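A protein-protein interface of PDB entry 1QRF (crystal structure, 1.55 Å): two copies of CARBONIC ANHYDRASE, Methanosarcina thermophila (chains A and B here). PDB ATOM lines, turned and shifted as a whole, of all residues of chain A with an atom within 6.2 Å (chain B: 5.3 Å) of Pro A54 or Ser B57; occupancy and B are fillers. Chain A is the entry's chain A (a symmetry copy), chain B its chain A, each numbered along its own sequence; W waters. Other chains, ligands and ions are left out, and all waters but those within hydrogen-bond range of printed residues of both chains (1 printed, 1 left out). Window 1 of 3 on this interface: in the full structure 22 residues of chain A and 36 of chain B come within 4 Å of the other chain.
Water W1 bridges OG of Ser A53 and NH1 of Arg B59.
Met A55 touches its own counterpart, Met B55.
Met A55 touches Ala B56, but with the chains exchanged Ala A56 does not touch Met B55 (7.7 Å).
4 positions are printed for both chains.
Of the 11 pairs that touch across the chains among the printed residues, 1 has its exchanged pair printed and touching as well.
The backbone carbonyl oxygen (O) of Pro A54 sits at hydrogen-bond distance from the backbone NH (N) of Gly A77 (3.3 Å).
N of Met A55 is in hydrogen-bond range of O of Gln A37, 2.8 Å away.
The backbone NH (N) of Gln A37 sits at hydrogen-bond distance from the side-chain carboxylate (OD2) of Asp A35, 2.8 Å away.
The backbone carbonyl oxygen of Val A52 is in hydrogen-bond range of the backbone NH of Asp A35, 2.9 Å away.
N of Leu B80 is in hydrogen-bond range of O of Ser B57 (2.9 Å).
The backbone NH of Ser A53 lies within hydrogen-bond range of the backbone carbonyl oxygen of Val A74 (2.9 Å).
The side-chain hydroxyl of Ser B57 is in hydrogen-bond range of the side-chain carboxylate of Asp A76 (2.7 Å).
The side-chain hydroxyl (OG) of Ser B39 lies close to the side-chain amide oxygen (OE1) of Gln A37 (3.5 Å).
The guanidinium group (NH1) of Arg B12 lies within salt-bridge range of the side-chain carboxylate (OD1) of Asp A35, 2.7 Å away.
OG of Ser A53 sits at hydrogen-bond distance from NH2 of Arg B59 (3.4 Å).
The guanidinium group (NH2) of Arg B59 lies within salt-bridge range of the side-chain carboxylate (OD1) of Asp A76 (2.8 Å).
Printed residues of chain A that touch a printed residue of chain B: Asp A35, Gln A37, Ser A53, Pro A54, Met A55 and Asp A76.
Hydrophobic or aromatic side chains of chain A within 4 Å of the printed part of chain B: Pro A54 and Met A55.
Of the 12 printed residues of chain B, 7 touch a printed residue of chain A.
Printed residues of chain B that touch a printed residue of chain A: Arg B12, Ser B39, Met B55, Ala B56, Ser B57, Arg B59 and Val B79.
Hydrophobic or aromatic side chains of chain B within 4 Å of the printed part of chain A: Val B79.
Among the printed residues, 11 pairs touch across the chains.
Among the printed residues, Asp or Glu carboxylates within 4 Å of a Lys or Arg side-chain nitrogen of the other chain: Asp A35 with Arg B12 (2.7 Å) and Asp A76 with Arg B59 (2.8 Å).
Pro A54 touches just these residues of chain B: Ser B39 and Ser B57.
Of chain A, only Pro A54 (3.7 Å) and Asp A76 (2.7 Å) come within 4 Å of Ser B57.
Printed residues of chain B within 4 Å of Met A55: Ser B39, Met B55 and Ala B56.
Of the printed residues of chain B, Asp A76 touches Ser B57, Arg B59 and Val B79.
Of the printed residues of chain A, Val B79 touches Asp A76.
Of the printed residues of chain A, Arg B12 touches Asp A35.
Of the printed residues of chain A, Met B55 touches Met A55 (3.3 Å).
The nearest residue of chain B that does not touch Pro A54 is Ile B41 (4.1 Å).
Among the printed residues, merely in contact across the chains: Pro A54 with Ser B39 (3.7 Å), Pro A54 with Ser B57 (3.7 Å), Met A55 with Ser B39 (3.7 Å), Met A55 with Met B55 (3.3 Å), Met A55 with Ala B56 (3.5 Å) and Asp A76 with Val B79 (3.9 Å).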
ATOM      1  N   ASP A  35      10.011 -23.806 -13.701  1.00  0.00           N
ATOM      2  CA  ASP A  35      10.278 -22.701 -14.643  1.00  0.00           C
ATOM      3  C   ASP A  35      11.748 -22.423 -14.678  1.00  0.00           C
ATOM      4  O   ASP A  35      12.479 -22.471 -13.689  1.00  0.00           O
ATOM      5  CB  ASP A  35       9.459 -21.487 -14.167  1.00  0.00           C
ATOM      6  CG  ASP A  35       9.504 -20.395 -15.232  1.00  0.00           C
ATOM      7  OD1 ASP A  35       8.604 -20.477 -16.110  1.00  0.00           O
ATOM      8  OD2 ASP A  35      10.367 -19.531 -15.146  1.00  0.00           O
ATOM      9  N   GLN A  37      13.159 -19.603 -14.663  1.00  0.00           N
ATOM     10  CA  GLN A  37      13.451 -18.511 -13.751  1.00  0.00           C
ATOM     11  C   GLN A  37      12.989 -18.795 -12.331  1.00  0.00           C
ATOM     12  O   GLN A  37      12.875 -17.864 -11.513  1.00  0.00           O
ATOM     13  CB  GLN A  37      12.886 -17.159 -14.245  1.00  0.00           C
ATOM     14  CG  GLN A  37      13.610 -16.772 -15.540  1.00  0.00           C
ATOM     15  CD  GLN A  37      12.909 -15.671 -16.336  1.00  0.00           C
ATOM     16  OE1 GLN A  37      11.814 -15.878 -16.864  1.00  0.00           O
ATOM     17  NE2 GLN A  37      13.422 -14.552 -16.512  1.00  0.00           N
ATOM     18  N   ALA A  38      12.786 -20.052 -11.959  1.00  0.00           N
ATOM     19  CA  ALA A  38      12.634 -20.475 -10.578  1.00  0.00           C
ATOM     20  C   ALA A  38      14.001 -20.970 -10.111  1.00  0.00           C
ATOM     21  O   ALA A  38      14.864 -21.256 -10.973  1.00  0.00           O
ATOM     22  CB  ALA A  38      11.581 -21.564 -10.384  1.00  0.00           C
ATOM     23  N   VAL A  52       6.215 -25.221 -10.602  1.00  0.00           N
ATOM     24  CA  VAL A  52       6.992 -24.223  -9.870  1.00  0.00           C
ATOM     25  C   VAL A  52       7.172 -23.051 -10.829  1.00  0.00           C
ATOM     26  O   VAL A  52       7.851 -23.221 -11.868  1.00  0.00           O
ATOM     27  CB  VAL A  52       8.313 -24.753  -9.391  1.00  0.00           C
ATOM     28  CG1 VAL A  52       9.060 -23.688  -8.569  1.00  0.00           C
ATOM     29  CG2 VAL A  52       8.162 -25.962  -8.478  1.00  0.00           C
ATOM     30  N   SER A  53       6.567 -21.949 -10.479  1.00  0.00           N
ATOM     31  CA  SER A  53       6.533 -20.761 -11.371  1.00  0.00           C
ATOM     32  C   SER A  53       7.723 -19.817 -11.310  1.00  0.00           C
ATOM     33  O   SER A  53       8.603 -19.956 -10.492  1.00  0.00           O
ATOM     34  CB  SER A  53       5.284 -19.939 -10.950  1.00  0.00           C
ATOM     35  OG  SER A  53       4.065 -20.657 -11.144  1.00  0.00           O
ATOM     36  N   PRO A  54       7.755 -18.890 -12.253  1.00  0.00           N
ATOM     37  CA  PRO A  54       8.843 -17.911 -12.318  1.00  0.00           C
ATOM     38  C   PRO A  54       9.094 -17.260 -10.976  1.00  0.00           C
ATOM     39  O   PRO A  54       8.124 -16.832 -10.331  1.00  0.00           O
ATOM     40  CB  PRO A  54       8.459 -16.873 -13.364  1.00  0.00           C
ATOM     41  CG  PRO A  54       7.522 -17.663 -14.253  1.00  0.00           C
ATOM     42  CD  PRO A  54       6.789 -18.635 -13.320  1.00  0.00           C
ATOM     43  N   MET A  55      10.367 -17.066 -10.616  1.00  0.00           N
ATOM     44  CA  MET A  55      10.728 -16.252  -9.445  1.00  0.00           C
ATOM     45  C   MET A  55      10.455 -16.935  -8.101  1.00  0.00           C
ATOM     46  O   MET A  55      10.787 -16.379  -7.034  1.00  0.00           O
ATOM     47  CB  MET A  55      10.140 -14.852  -9.468  1.00  0.00           C
ATOM     48  CG  MET A  55      10.177 -14.048 -10.748  1.00  0.00           C
ATOM     49  SD  MET A  55      11.815 -14.029 -11.535  1.00  0.00           S
ATOM     50  CE  MET A  55      11.255 -13.467 -13.142  1.00  0.00           C
ATOM     51  N   ALA A  56       9.991 -18.173  -8.119  1.00  0.00           N
ATOM     52  CA  ALA A  56       9.919 -18.957  -6.874  1.00  0.00           C
ATOM     53  C   ALA A  56      11.313 -19.359  -6.472  1.00  0.00           C
ATOM     54  O   ALA A  56      12.170 -19.611  -7.335  1.00  0.00           O
ATOM     55  CB  ALA A  56       9.005 -20.160  -7.098  1.00  0.00           C
ATOM     56  N   VAL A  74       3.712 -24.151  -6.579  1.00  0.00           N
ATOM     57  CA  VAL A  74       4.573 -23.143  -5.890  1.00  0.00           C
ATOM     58  C   VAL A  74       4.618 -21.945  -6.852  1.00  0.00           C
ATOM     59  O   VAL A  74       5.311 -22.038  -7.870  1.00  0.00           O
ATOM     60  CB  VAL A  74       5.942 -23.742  -5.661  1.00  0.00           C
ATOM     61  CG1 VAL A  74       6.879 -22.711  -4.982  1.00  0.00           C
ATOM     62  CG2 VAL A  74       5.895 -25.026  -4.811  1.00  0.00           C
ATOM     63  N   GLN A  75       3.778 -20.979  -6.606  1.00  0.00           N
ATOM     64  CA  GLN A  75       3.566 -19.887  -7.549  1.00  0.00           C
ATOM     65  C   GLN A  75       4.648 -18.827  -7.530  1.00  0.00           C
ATOM     66  O   GLN A  75       5.649 -18.909  -6.842  1.00  0.00           O
ATOM     67  CB  GLN A  75       2.109 -19.352  -7.393  1.00  0.00           C
ATOM     68  CG  GLN A  75       1.067 -20.458  -7.669  1.00  0.00           C
ATOM     69  CD  GLN A  75      -0.329 -19.892  -7.512  1.00  0.00           C
ATOM     70  OE1 GLN A  75      -0.589 -18.688  -7.619  1.00  0.00           O
ATOM     71  NE2 GLN A  75      -1.268 -20.820  -7.253  1.00  0.00           N
ATOM     72  N   ASP A  76       4.402 -17.801  -8.368  1.00  0.00           N
ATOM     73  CA  ASP A  76       5.455 -16.829  -8.684  1.00  0.00           C
ATOM     74  C   ASP A  76       5.909 -16.090  -7.441  1.00  0.00           C
ATOM     75  O   ASP A  76       5.119 -15.619  -6.641  1.00  0.00           O
ATOM     76  CB  ASP A  76       4.986 -15.761  -9.688  1.00  0.00           C
ATOM     77  CG  ASP A  76       4.156 -16.289 -10.855  1.00  0.00           C
ATOM     78  OD1 ASP A  76       3.077 -16.857 -10.577  1.00  0.00           O
ATOM     79  OD2 ASP A  76       4.597 -16.157 -12.027  1.00  0.00           O
ATOM     80  N   GLY A  77       7.224 -16.096  -7.216  1.00  0.00           N
ATOM     81  CA  GLY A  77       7.776 -15.354  -6.086  1.00  0.00           C
ATOM     82  C   GLY A  77       7.612 -16.047  -4.773  1.00  0.00           C
ATOM     83  O   GLY A  77       7.959 -15.385  -3.739  1.00  0.00           O
ATOM     84  N   VAL A  78       7.070 -17.265  -4.706  1.00  0.00           N
ATOM     85  CA  VAL A  78       6.961 -17.934  -3.410  1.00  0.00           C
ATOM     86  C   VAL A  78       8.328 -18.322  -2.880  1.00  0.00           C
ATOM     87  O   VAL A  78       9.169 -18.688  -3.717  1.00  0.00           O
ATOM     88  CB  VAL A  78       6.072 -19.171  -3.547  1.00  0.00           C
ATOM     89  CG1 VAL A  78       6.065 -20.107  -2.312  1.00  0.00           C
ATOM     90  CG2 VAL A  78       4.633 -18.744  -3.789  1.00  0.00           C
ATOM     91  N   ARG B  12       7.929 -15.099 -23.535  1.00  0.00           N
ATOM     92  CA  ARG B  12       7.530 -16.385 -24.064  1.00  0.00           C
ATOM     93  C   ARG B  12       6.031 -16.507 -24.307  1.00  0.00           C
ATOM     94  O   ARG B  12       5.215 -15.779 -23.729  1.00  0.00           O
ATOM     95  CB  ARG B  12       7.785 -17.432 -22.937  1.00  0.00           C
ATOM     96  CG  ARG B  12       9.188 -17.601 -22.413  1.00  0.00           C
ATOM     97  CD  ARG B  12       9.260 -17.953 -20.928  1.00  0.00           C
ATOM     98  NE  ARG B  12       8.724 -19.286 -20.717  1.00  0.00           N
ATOM     99  CZ  ARG B  12       8.727 -19.973 -19.588  1.00  0.00           C
ATOM    100  NH1 ARG B  12       9.228 -19.458 -18.483  1.00  0.00           N
ATOM    101  NH2 ARG B  12       8.207 -21.191 -19.597  1.00  0.00           N
ATOM    102  N   SER B  39      10.016 -11.837 -16.205  1.00  0.00           N
ATOM    103  CA  SER B  39       9.369 -12.884 -16.969  1.00  0.00           C
ATOM    104  C   SER B  39       8.080 -12.365 -17.538  1.00  0.00           C
ATOM    105  O   SER B  39       7.288 -11.863 -16.720  1.00  0.00           O
ATOM    106  CB  SER B  39       9.029 -14.101 -16.085  1.00  0.00           C
ATOM    107  OG  SER B  39       8.416 -15.152 -16.796  1.00  0.00           O
ATOM    108  N   ILE B  41       4.976 -13.770 -19.904  1.00  0.00           N
ATOM    109  CA  ILE B  41       4.465 -14.938 -20.612  1.00  0.00           C
ATOM    110  C   ILE B  41       3.035 -14.764 -21.075  1.00  0.00           C
ATOM    111  O   ILE B  41       2.168 -14.326 -20.337  1.00  0.00           O
ATOM    112  CB  ILE B  41       4.452 -16.143 -19.620  1.00  0.00           C
ATOM    113  CG1 ILE B  41       5.844 -16.550 -19.155  1.00  0.00           C
ATOM    114  CG2 ILE B  41       3.726 -17.358 -20.220  1.00  0.00           C
ATOM    115  CD1 ILE B  41       5.825 -17.512 -17.971  1.00  0.00           C
ATOM    116  N   MET B  55      12.841  -9.432 -11.684  1.00  0.00           N
ATOM    117  CA  MET B  55      12.060 -10.294 -10.785  1.00  0.00           C
ATOM    118  C   MET B  55      10.546 -10.072 -10.864  1.00  0.00           C
ATOM    119  O   MET B  55       9.768 -10.793 -10.206  1.00  0.00           O
ATOM    120  CB  MET B  55      12.535 -10.265  -9.342  1.00  0.00           C
ATOM    121  CG  MET B  55      14.015 -10.330  -9.043  1.00  0.00           C
ATOM    122  SD  MET B  55      14.868 -11.666  -9.933  1.00  0.00           S
ATOM    123  CE  MET B  55      16.528 -11.033  -9.693  1.00  0.00           C
ATOM    124  N   ALA B  56      10.095  -9.196 -11.746  1.00  0.00           N
ATOM    125  CA  ALA B  56       8.651  -9.099 -12.024  1.00  0.00           C
ATOM    126  C   ALA B  56       8.229 -10.302 -12.825  1.00  0.00           C
ATOM    127  O   ALA B  56       9.004 -10.813 -13.651  1.00  0.00           O
ATOM    128  CB  ALA B  56       8.374  -7.785 -12.752  1.00  0.00           C
ATOM    129  N   SER B  57       7.012 -10.746 -12.576  1.00  0.00           N
ATOM    130  CA  SER B  57       6.405 -11.849 -13.301  1.00  0.00           C
ATOM    131  C   SER B  57       5.060 -11.483 -13.824  1.00  0.00           C
ATOM    132  O   SER B  57       4.132 -11.323 -13.029  1.00  0.00           O
ATOM    133  CB  SER B  57       6.467 -13.155 -12.514  1.00  0.00           C
ATOM    134  OG  SER B  57       5.951 -14.198 -13.323  1.00  0.00           O
ATOM    135  N   ILE B  58       4.926 -11.401 -15.130  1.00  0.00           N
ATOM    136  CA  ILE B  58       3.634 -11.088 -15.774  1.00  0.00           C
ATOM    137  C   ILE B  58       3.249 -12.364 -16.517  1.00  0.00           C
ATOM    138  O   ILE B  58       3.961 -12.748 -17.445  1.00  0.00           O
ATOM    139  CB  ILE B  58       3.758  -9.915 -16.761  1.00  0.00           C
ATOM    140  CG1 ILE B  58       4.226  -8.647 -16.030  1.00  0.00           C
ATOM    141  CG2 ILE B  58       2.387  -9.725 -17.447  1.00  0.00           C
ATOM    142  CD1 ILE B  58       4.457  -7.504 -17.031  1.00  0.00           C
ATOM    143  N   ARG B  59       2.232 -13.071 -16.018  1.00  0.00           N
ATOM    144  CA  ARG B  59       1.913 -14.389 -16.515  1.00  0.00           C
ATOM    145  C   ARG B  59       0.463 -14.488 -16.940  1.00  0.00           C
ATOM    146  O   ARG B  59      -0.403 -14.563 -16.075  1.00  0.00           O
ATOM    147  CB  ARG B  59       2.292 -15.435 -15.449  1.00  0.00           C
ATOM    148  CG  ARG B  59       2.203 -16.870 -15.971  1.00  0.00           C
ATOM    149  CD  ARG B  59       3.026 -17.848 -15.112  1.00  0.00           C
ATOM    150  NE  ARG B  59       2.581 -17.899 -13.693  1.00  0.00           N
ATOM    151  CZ  ARG B  59       1.701 -18.742 -13.147  1.00  0.00           C
ATOM    152  NH1 ARG B  59       1.068 -19.657 -13.895  1.00  0.00           N
ATOM    153  NH2 ARG B  59       1.423 -18.696 -11.838  1.00  0.00           N
ATOM    154  N   GLY B  77       9.795  -7.620  -8.550  1.00  0.00           N
ATOM    155  CA  GLY B  77       9.040  -8.622  -7.803  1.00  0.00           C
ATOM    156  C   GLY B  77       7.559  -8.489  -7.945  1.00  0.00           C
ATOM    157  O   GLY B  77       6.851  -9.256  -7.212  1.00  0.00           O
ATOM    158  N   VAL B  78       7.030  -7.567  -8.753  1.00  0.00           N
ATOM    159  CA  VAL B  78       5.577  -7.489  -8.902  1.00  0.00           C
ATOM    160  C   VAL B  78       5.039  -8.698  -9.642  1.00  0.00           C
ATOM    161  O   VAL B  78       5.749  -9.159 -10.550  1.00  0.00           O
ATOM    162  CB  VAL B  78       5.209  -6.202  -9.643  1.00  0.00           C
ATOM    163  CG1 VAL B  78       3.726  -6.107 -10.082  1.00  0.00           C
ATOM    164  CG2 VAL B  78       5.487  -5.001  -8.754  1.00  0.00           C
ATOM    165  N   VAL B  79       3.866  -9.167  -9.266  1.00  0.00           N
ATOM    166  CA  VAL B  79       3.292 -10.292 -10.015  1.00  0.00           C
ATOM    167  C   VAL B  79       1.977  -9.813 -10.622  1.00  0.00           C
ATOM    168  O   VAL B  79       1.155  -9.234  -9.916  1.00  0.00           O
ATOM    169  CB  VAL B  79       3.080 -11.497  -9.101  1.00  0.00           C
ATOM    170  CG1 VAL B  79       2.250 -12.641  -9.731  1.00  0.00           C
ATOM    171  CG2 VAL B  79       4.444 -12.068  -8.696  1.00  0.00           C
ATOM    172  N   LEU B  80       1.685 -10.174 -11.857  1.00  0.00           N
ATOM    173  CA  LEU B  80       0.392 -10.032 -12.511  1.00  0.00           C
ATOM    174  C   LEU B  80      -0.024 -11.428 -12.965  1.00  0.00           C
ATOM    175  O   LEU B  80       0.729 -12.117 -13.677  1.00  0.00           O
ATOM    176  CB  LEU B  80       0.404  -9.074 -13.726  1.00  0.00           C
ATOM    177  CG  LEU B  80       0.889  -7.655 -13.466  1.00  0.00           C
ATOM    178  CD1 LEU B  80       0.805  -6.924 -14.825  1.00  0.00           C
ATOM    179  CD2 LEU B  80       0.002  -7.013 -12.403  1.00  0.00           C
HETATM  180  O   HOH W   1       4.119 -20.903 -13.732  1.00  0.00           O
